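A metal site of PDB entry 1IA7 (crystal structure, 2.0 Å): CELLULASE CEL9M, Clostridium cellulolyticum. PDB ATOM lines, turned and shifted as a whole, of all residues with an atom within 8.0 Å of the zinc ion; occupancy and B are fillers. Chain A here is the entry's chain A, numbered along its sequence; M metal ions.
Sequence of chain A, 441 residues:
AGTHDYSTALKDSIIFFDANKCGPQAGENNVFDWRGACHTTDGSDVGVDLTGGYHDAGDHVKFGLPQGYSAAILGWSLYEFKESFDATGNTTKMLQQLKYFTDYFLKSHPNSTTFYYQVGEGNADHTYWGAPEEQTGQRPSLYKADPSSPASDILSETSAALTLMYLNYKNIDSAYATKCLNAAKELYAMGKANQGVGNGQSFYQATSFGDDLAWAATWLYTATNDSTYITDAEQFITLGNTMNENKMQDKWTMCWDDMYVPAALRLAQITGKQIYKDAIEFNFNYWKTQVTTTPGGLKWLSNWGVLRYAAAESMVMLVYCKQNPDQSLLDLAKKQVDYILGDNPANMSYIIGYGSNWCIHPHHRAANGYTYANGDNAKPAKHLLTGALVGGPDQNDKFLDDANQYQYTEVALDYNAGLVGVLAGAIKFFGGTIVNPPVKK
The backbone carbonyl oxygen (O) of Cys 38 lies within hydrogen-bond range of the backbone NH (N) of Gly 23 (3.1 Å). O of Asn 20 lies within hydrogen-bond range of N of His 55 (2.8 Å). NH2 of Arg 139 lies close to SG of Cys 22 (3.8 Å). A ring nitrogen (NE2) of His 39 sits at hydrogen-bond distance from the side-chain amide oxygen of Gln 135. SG of Cys 38 lies close to NH2 of Arg 35 (3.3 Å). The side-chain hydroxyl (OH) of Tyr 100 sits at hydrogen-bond distance from the backbone carbonyl oxygen (O) of Cys 22 (2.7 Å). O of Gly 53 sits at hydrogen-bond distance from N of Cys 22 (3.0 Å).
The zinc ion is bound by ND1 of His 39 (2.0 Å), NE2 of His 55 (2.1 Å), SG of Cys 22 (2.3 Å) and SG of Cys 38 (2.4 Å).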
ATOM      1  N   ASN A  20     -33.498  22.504   8.665  1.00  0.00           N
ATOM      2  CA  ASN A  20     -32.079  22.811   8.453  1.00  0.00           C
ATOM      3  C   ASN A  20     -31.499  22.357   7.115  1.00  0.00           C
ATOM      4  O   ASN A  20     -30.293  22.511   6.883  1.00  0.00           O
ATOM      5  CB  ASN A  20     -31.257  22.218   9.604  1.00  0.00           C
ATOM      6  CG  ASN A  20     -31.363  23.039  10.875  1.00  0.00           C
ATOM      7  OD1 ASN A  20     -32.435  23.544  11.206  1.00  0.00           O
ATOM      8  ND2 ASN A  20     -30.261  23.170  11.610  1.00  0.00           N
ATOM      9  N   LYS A  21     -32.322  21.810   6.231  1.00  0.00           N
ATOM     10  CA  LYS A  21     -31.823  21.374   4.933  1.00  0.00           C
ATOM     11  C   LYS A  21     -31.180  22.535   4.190  1.00  0.00           C
ATOM     12  O   LYS A  21     -31.672  23.667   4.211  1.00  0.00           O
ATOM     13  CB  LYS A  21     -32.960  20.751   4.102  1.00  0.00           C
ATOM     14  CG  LYS A  21     -33.309  19.342   4.547  1.00  0.00           C
ATOM     15  CD  LYS A  21     -34.443  18.730   3.745  1.00  0.00           C
ATOM     16  CE  LYS A  21     -34.776  17.342   4.280  1.00  0.00           C
ATOM     17  NZ  LYS A  21     -35.967  16.735   3.612  1.00  0.00           N
ATOM     18  N   CYS A  22     -30.058  22.248   3.539  1.00  0.00           N
ATOM     19  CA  CYS A  22     -29.297  23.251   2.814  1.00  0.00           C
ATOM     20  C   CYS A  22     -29.167  22.830   1.349  1.00  0.00           C
ATOM     21  O   CYS A  22     -29.160  21.638   1.049  1.00  0.00           O
ATOM     22  CB  CYS A  22     -27.906  23.374   3.465  1.00  0.00           C
ATOM     23  SG  CYS A  22     -26.801  24.666   2.835  1.00  0.00           S
ATOM     24  N   GLY A  23     -29.066  23.809   0.460  1.00  0.00           N
ATOM     25  CA  GLY A  23     -28.904  23.495  -0.950  1.00  0.00           C
ATOM     26  C   GLY A  23     -30.087  23.816  -1.853  1.00  0.00           C
ATOM     27  O   GLY A  23     -31.166  24.203  -1.380  1.00  0.00           O
ATOM     28  N   PRO A  24     -29.922  23.641  -3.164  1.00  0.00           N
ATOM     29  CA  PRO A  24     -30.990  23.914  -4.138  1.00  0.00           C
ATOM     30  C   PRO A  24     -32.217  23.019  -4.001  1.00  0.00           C
ATOM     31  O   PRO A  24     -33.289  23.379  -4.481  1.00  0.00           O
ATOM     32  CB  PRO A  24     -30.275  23.738  -5.483  1.00  0.00           C
ATOM     33  CG  PRO A  24     -29.223  22.729  -5.186  1.00  0.00           C
ATOM     34  CD  PRO A  24     -28.686  23.201  -3.851  1.00  0.00           C
ATOM     35  N   ALA A  26     -33.317  21.940  -0.968  1.00  0.00           N
ATOM     36  CA  ALA A  26     -33.782  22.063   0.407  1.00  0.00           C
ATOM     37  C   ALA A  26     -35.295  22.097   0.562  1.00  0.00           C
ATOM     38  O   ALA A  26     -35.836  21.526   1.506  1.00  0.00           O
ATOM     39  CB  ALA A  26     -33.149  23.296   1.066  1.00  0.00           C
ATOM     40  N   ARG A  35     -39.202  27.316   4.104  1.00  0.00           N
ATOM     41  CA  ARG A  35     -37.843  26.928   3.721  1.00  0.00           C
ATOM     42  C   ARG A  35     -37.734  26.798   2.211  1.00  0.00           C
ATOM     43  O   ARG A  35     -38.628  26.259   1.555  1.00  0.00           O
ATOM     44  CB  ARG A  35     -37.431  25.593   4.361  1.00  0.00           C
ATOM     45  CG  ARG A  35     -36.960  25.674   5.819  1.00  0.00           C
ATOM     46  CD  ARG A  35     -35.964  26.818   6.032  1.00  0.00           C
ATOM     47  NE  ARG A  35     -35.010  26.949   4.927  1.00  0.00           N
ATOM     48  CZ  ARG A  35     -34.005  26.112   4.706  1.00  0.00           C
ATOM     49  NH1 ARG A  35     -33.804  25.076   5.515  1.00  0.00           N
ATOM     50  NH2 ARG A  35     -33.212  26.296   3.666  1.00  0.00           N
ATOM     51  N   GLY A  36     -36.626  27.298   1.662  1.00  0.00           N
ATOM     52  CA  GLY A  36     -36.399  27.222   0.229  1.00  0.00           C
ATOM     53  C   GLY A  36     -34.930  26.995  -0.074  1.00  0.00           C
ATOM     54  O   GLY A  36     -34.119  26.806   0.841  1.00  0.00           O
ATOM     55  N   ALA A  37     -34.583  27.025  -1.356  1.00  0.00           N
ATOM     56  CA  ALA A  37     -33.201  26.830  -1.795  1.00  0.00           C
ATOM     57  C   ALA A  37     -32.244  27.835  -1.128  1.00  0.00           C
ATOM     58  O   ALA A  37     -32.582  29.013  -0.980  1.00  0.00           O
ATOM     59  CB  ALA A  37     -33.115  26.954  -3.301  1.00  0.00           C
ATOM     60  N   CYS A  38     -31.060  27.368  -0.751  1.00  0.00           N
ATOM     61  CA  CYS A  38     -30.065  28.223  -0.112  1.00  0.00           C
ATOM     62  C   CYS A  38     -28.630  27.741  -0.346  1.00  0.00           C
ATOM     63  O   CYS A  38     -28.414  26.569  -0.664  1.00  0.00           O
ATOM     64  CB  CYS A  38     -30.334  28.297   1.403  1.00  0.00           C
ATOM     65  SG  CYS A  38     -30.199  26.711   2.272  1.00  0.00           S
ATOM     66  N   HIS A  39     -27.667  28.662  -0.207  1.00  0.00           N
ATOM     67  CA  HIS A  39     -26.245  28.359  -0.377  1.00  0.00           C
ATOM     68  C   HIS A  39     -26.055  27.398  -1.548  1.00  0.00           C
ATOM     69  O   HIS A  39     -25.369  26.378  -1.444  1.00  0.00           O
ATOM     70  CB  HIS A  39     -25.694  27.749   0.913  1.00  0.00           C
ATOM     71  CG  HIS A  39     -26.024  28.538   2.139  1.00  0.00           C
ATOM     72  ND1 HIS A  39     -26.957  28.131   3.057  1.00  0.00           N
ATOM     73  CD2 HIS A  39     -25.561  29.728   2.582  1.00  0.00           C
ATOM     74  CE1 HIS A  39     -27.071  29.038   4.010  1.00  0.00           C
ATOM     75  NE2 HIS A  39     -26.227  30.016   3.745  1.00  0.00           N
ATOM     76  N   THR A  40     -26.638  27.771  -2.679  1.00  0.00           N
ATOM     77  CA  THR A  40     -26.612  26.953  -3.885  1.00  0.00           C
ATOM     78  C   THR A  40     -25.312  26.852  -4.666  1.00  0.00           C
ATOM     79  O   THR A  40     -25.247  26.153  -5.672  1.00  0.00           O
ATOM     80  CB  THR A  40     -27.731  27.397  -4.830  1.00  0.00           C
ATOM     81  OG1 THR A  40     -27.521  28.761  -5.219  1.00  0.00           O
ATOM     82  CG2 THR A  40     -29.078  27.276  -4.133  1.00  0.00           C
ATOM     83  N   ASP A  42     -22.245  26.322  -2.900  1.00  0.00           N
ATOM     84  CA  ASP A  42     -21.278  25.770  -1.957  1.00  0.00           C
ATOM     85  C   ASP A  42     -20.261  24.895  -2.681  1.00  0.00           C
ATOM     86  O   ASP A  42     -20.629  24.037  -3.498  1.00  0.00           O
ATOM     87  CB  ASP A  42     -21.983  24.914  -0.881  1.00  0.00           C
ATOM     88  CG  ASP A  42     -22.629  25.761   0.209  1.00  0.00           C
ATOM     89  OD1 ASP A  42     -22.396  26.980   0.264  1.00  0.00           O
ATOM     90  OD2 ASP A  42     -23.373  25.180   1.038  1.00  0.00           O
ATOM     91  N   GLY A  52     -26.035  20.794  -0.439  1.00  0.00           N
ATOM     92  CA  GLY A  52     -26.765  19.726   0.225  1.00  0.00           C
ATOM     93  C   GLY A  52     -26.389  19.648   1.684  1.00  0.00           C
ATOM     94  O   GLY A  52     -25.739  20.556   2.208  1.00  0.00           O
ATOM     95  N   GLY A  53     -26.759  18.561   2.353  1.00  0.00           N
ATOM     96  CA  GLY A  53     -26.427  18.446   3.761  1.00  0.00           C
ATOM     97  C   GLY A  53     -27.314  19.348   4.603  1.00  0.00           C
ATOM     98  O   GLY A  53     -28.354  19.802   4.126  1.00  0.00           O
ATOM     99  N   TYR A  54     -26.898  19.628   5.832  1.00  0.00           N
ATOM    100  CA  TYR A  54     -27.698  20.446   6.735  1.00  0.00           C
ATOM    101  C   TYR A  54     -26.957  21.535   7.500  1.00  0.00           C
ATOM    102  O   TYR A  54     -25.776  21.393   7.840  1.00  0.00           O
ATOM    103  CB  TYR A  54     -28.364  19.558   7.802  1.00  0.00           C
ATOM    104  CG  TYR A  54     -29.300  18.492   7.283  1.00  0.00           C
ATOM    105  CD1 TYR A  54     -28.805  17.318   6.701  1.00  0.00           C
ATOM    106  CD2 TYR A  54     -30.678  18.624   7.435  1.00  0.00           C
ATOM    107  CE1 TYR A  54     -29.683  16.305   6.286  1.00  0.00           C
ATOM    108  CE2 TYR A  54     -31.555  17.625   7.039  1.00  0.00           C
ATOM    109  CZ  TYR A  54     -31.050  16.467   6.466  1.00  0.00           C
ATOM    110  OH  TYR A  54     -31.923  15.474   6.107  1.00  0.00           O
ATOM    111  N   HIS A  55     -27.665  22.626   7.792  1.00  0.00           N
ATOM    112  CA  HIS A  55     -27.100  23.701   8.598  1.00  0.00           C
ATOM    113  C   HIS A  55     -26.939  23.019   9.948  1.00  0.00           C
ATOM    114  O   HIS A  55     -27.789  22.230  10.352  1.00  0.00           O
ATOM    115  CB  HIS A  55     -28.100  24.853   8.718  1.00  0.00           C
ATOM    116  CG  HIS A  55     -28.491  25.451   7.409  1.00  0.00           C
ATOM    117  ND1 HIS A  55     -29.760  25.927   7.146  1.00  0.00           N
ATOM    118  CD2 HIS A  55     -27.778  25.636   6.262  1.00  0.00           C
ATOM    119  CE1 HIS A  55     -29.805  26.382   5.901  1.00  0.00           C
ATOM    120  NE2 HIS A  55     -28.621  26.214   5.345  1.00  0.00           N
ATOM    121  N   ASP A  59     -27.355  28.317  13.279  1.00  0.00           N
ATOM    122  CA  ASP A  59     -26.530  28.993  12.289  1.00  0.00           C
ATOM    123  C   ASP A  59     -26.598  28.221  10.979  1.00  0.00           C
ATOM    124  O   ASP A  59     -27.368  27.276  10.833  1.00  0.00           O
ATOM    125  CB  ASP A  59     -25.085  29.100  12.777  1.00  0.00           C
ATOM    126  CG  ASP A  59     -24.475  27.752  13.096  1.00  0.00           C
ATOM    127  OD1 ASP A  59     -25.192  26.732  13.007  1.00  0.00           O
ATOM    128  OD2 ASP A  59     -23.275  27.696  13.446  1.00  0.00           O
ATOM    129  N   HIS A  60     -25.758  28.608  10.013  1.00  0.00           N
ATOM    130  CA  HIS A  60     -25.803  27.959   8.711  1.00  0.00           C
ATOM    131  C   HIS A  60     -24.558  27.226   8.240  1.00  0.00           C
ATOM    132  O   HIS A  60     -24.542  26.696   7.136  1.00  0.00           O
ATOM    133  CB  HIS A  60     -26.243  28.986   7.676  1.00  0.00           C
ATOM    134  CG  HIS A  60     -27.592  29.566   7.968  1.00  0.00           C
ATOM    135  ND1 HIS A  60     -27.948  30.856   7.630  1.00  0.00           N
ATOM    136  CD2 HIS A  60     -28.687  29.034   8.567  1.00  0.00           C
ATOM    137  CE1 HIS A  60     -29.176  31.095   8.023  1.00  0.00           C
ATOM    138  NE2 HIS A  60     -29.649  30.004   8.596  1.00  0.00           N
ATOM    139  N   VAL A  61     -23.524  27.181   9.079  1.00  0.00           N
ATOM    140  CA  VAL A  61     -22.303  26.478   8.707  1.00  0.00           C
ATOM    141  C   VAL A  61     -22.556  24.974   8.737  1.00  0.00           C
ATOM    142  O   VAL A  61     -23.396  24.490   9.490  1.00  0.00           O
ATOM    143  CB  VAL A  61     -21.148  26.793   9.699  1.00  0.00           C
ATOM    144  CG1 VAL A  61     -19.920  25.956   9.355  1.00  0.00           C
ATOM    145  CG2 VAL A  61     -20.808  28.287   9.632  1.00  0.00           C
ATOM    146  N   LYS A  62     -21.830  24.241   7.909  1.00  0.00           N
ATOM    147  CA  LYS A  62     -21.953  22.786   7.887  1.00  0.00           C
ATOM    148  C   LYS A  62     -20.661  22.242   8.488  1.00  0.00           C
ATOM    149  O   LYS A  62     -19.636  22.171   7.804  1.00  0.00           O
ATOM    150  CB  LYS A  62     -22.180  22.287   6.454  1.00  0.00           C
ATOM    151  CG  LYS A  62     -23.486  22.827   5.852  1.00  0.00           C
ATOM    152  CD  LYS A  62     -23.823  22.233   4.491  1.00  0.00           C
ATOM    153  CE  LYS A  62     -22.889  22.735   3.408  1.00  0.00           C
ATOM    154  NZ  LYS A  62     -23.438  22.438   2.044  1.00  0.00           N
ATOM    155  N   TYR A 100     -30.644  12.560   2.424  1.00  0.00           N
ATOM    156  CA  TYR A 100     -30.231  13.942   2.211  1.00  0.00           C
ATOM    157  C   TYR A 100     -28.835  14.115   2.807  1.00  0.00           C
ATOM    158  O   TYR A 100     -28.018  14.914   2.321  1.00  0.00           O
ATOM    159  CB  TYR A 100     -31.200  14.925   2.864  1.00  0.00           C
ATOM    160  CG  TYR A 100     -31.203  16.286   2.181  1.00  0.00           C
ATOM    161  CD1 TYR A 100     -31.919  16.495   1.006  1.00  0.00           C
ATOM    162  CD2 TYR A 100     -30.448  17.347   2.678  1.00  0.00           C
ATOM    163  CE1 TYR A 100     -31.889  17.715   0.335  1.00  0.00           C
ATOM    164  CE2 TYR A 100     -30.417  18.582   2.027  1.00  0.00           C
ATOM    165  CZ  TYR A 100     -31.137  18.754   0.854  1.00  0.00           C
ATOM    166  OH  TYR A 100     -31.112  19.962   0.188  1.00  0.00           O
ATOM    167  N   ALA A 131     -32.667  34.997   6.839  1.00  0.00           N
ATOM    168  CA  ALA A 131     -33.014  33.734   6.220  1.00  0.00           C
ATOM    169  C   ALA A 131     -31.821  33.152   5.459  1.00  0.00           C
ATOM    170  O   ALA A 131     -31.051  33.873   4.830  1.00  0.00           O
ATOM    171  CB  ALA A 131     -34.192  33.924   5.267  1.00  0.00           C
ATOM    172  N   PRO A 132     -31.634  31.825   5.540  1.00  0.00           N
ATOM    173  CA  PRO A 132     -30.497  31.249   4.809  1.00  0.00           C
ATOM    174  C   PRO A 132     -30.644  31.440   3.302  1.00  0.00           C
ATOM    175  O   PRO A 132     -29.649  31.508   2.582  1.00  0.00           O
ATOM    176  CB  PRO A 132     -30.516  29.779   5.228  1.00  0.00           C
ATOM    177  CG  PRO A 132     -31.962  29.530   5.588  1.00  0.00           C
ATOM    178  CD  PRO A 132     -32.327  30.796   6.336  1.00  0.00           C
ATOM    179  N   GLU A 133     -31.881  31.551   2.836  1.00  0.00           N
ATOM    180  CA  GLU A 133     -32.147  31.748   1.411  1.00  0.00           C
ATOM    181  C   GLU A 133     -31.662  33.111   0.918  1.00  0.00           C
ATOM    182  O   GLU A 133     -31.474  33.312  -0.280  1.00  0.00           O
ATOM    183  CB  GLU A 133     -33.639  31.602   1.111  1.00  0.00           C
ATOM    184  CG  GLU A 133     -34.242  30.213   1.417  1.00  0.00           C
ATOM    185  CD  GLU A 133     -34.554  30.011   2.899  1.00  0.00           C
ATOM    186  OE1 GLU A 133     -34.267  30.919   3.716  1.00  0.00           O
ATOM    187  OE2 GLU A 133     -35.101  28.932   3.232  1.00  0.00           O
ATOM    188  N   GLN A 135     -28.840  34.741   2.436  1.00  0.00           N
ATOM    189  CA  GLN A 135     -27.448  34.955   2.827  1.00  0.00           C
ATOM    190  C   GLN A 135     -26.543  34.751   1.611  1.00  0.00           C
ATOM    191  O   GLN A 135     -26.071  33.646   1.355  1.00  0.00           O
ATOM    192  CB  GLN A 135     -27.063  33.990   3.958  1.00  0.00           C
ATOM    193  CG  GLN A 135     -25.627  34.106   4.441  1.00  0.00           C
ATOM    194  CD  GLN A 135     -25.366  33.259   5.693  1.00  0.00           C
ATOM    195  OE1 GLN A 135     -26.008  32.234   5.904  1.00  0.00           O
ATOM    196  NE2 GLN A 135     -24.401  33.687   6.511  1.00  0.00           N
ATOM    197  N   ARG A 139     -19.329  30.854   0.122  1.00  0.00           N
ATOM    198  CA  ARG A 139     -18.875  30.304   1.384  1.00  0.00           C
ATOM    199  C   ARG A 139     -17.581  29.545   1.135  1.00  0.00           C
ATOM    200  O   ARG A 139     -17.397  28.931   0.097  1.00  0.00           O
ATOM    201  CB  ARG A 139     -19.918  29.343   1.961  1.00  0.00           C
ATOM    202  CG  ARG A 139     -20.714  29.903   3.123  1.00  0.00           C
ATOM    203  CD  ARG A 139     -22.205  29.734   2.891  1.00  0.00           C
ATOM    204  NE  ARG A 139     -22.635  28.336   2.800  1.00  0.00           N
ATOM    205  CZ  ARG A 139     -23.134  27.627   3.814  1.00  0.00           C
ATOM    206  NH1 ARG A 139     -23.264  28.192   5.015  1.00  0.00           N
ATOM    207  NH2 ARG A 139     -23.559  26.393   3.617  1.00  0.00           N
HETATM  208 ZN    ZN M   1     -28.088  26.482   3.332  1.00  0.00          ZN
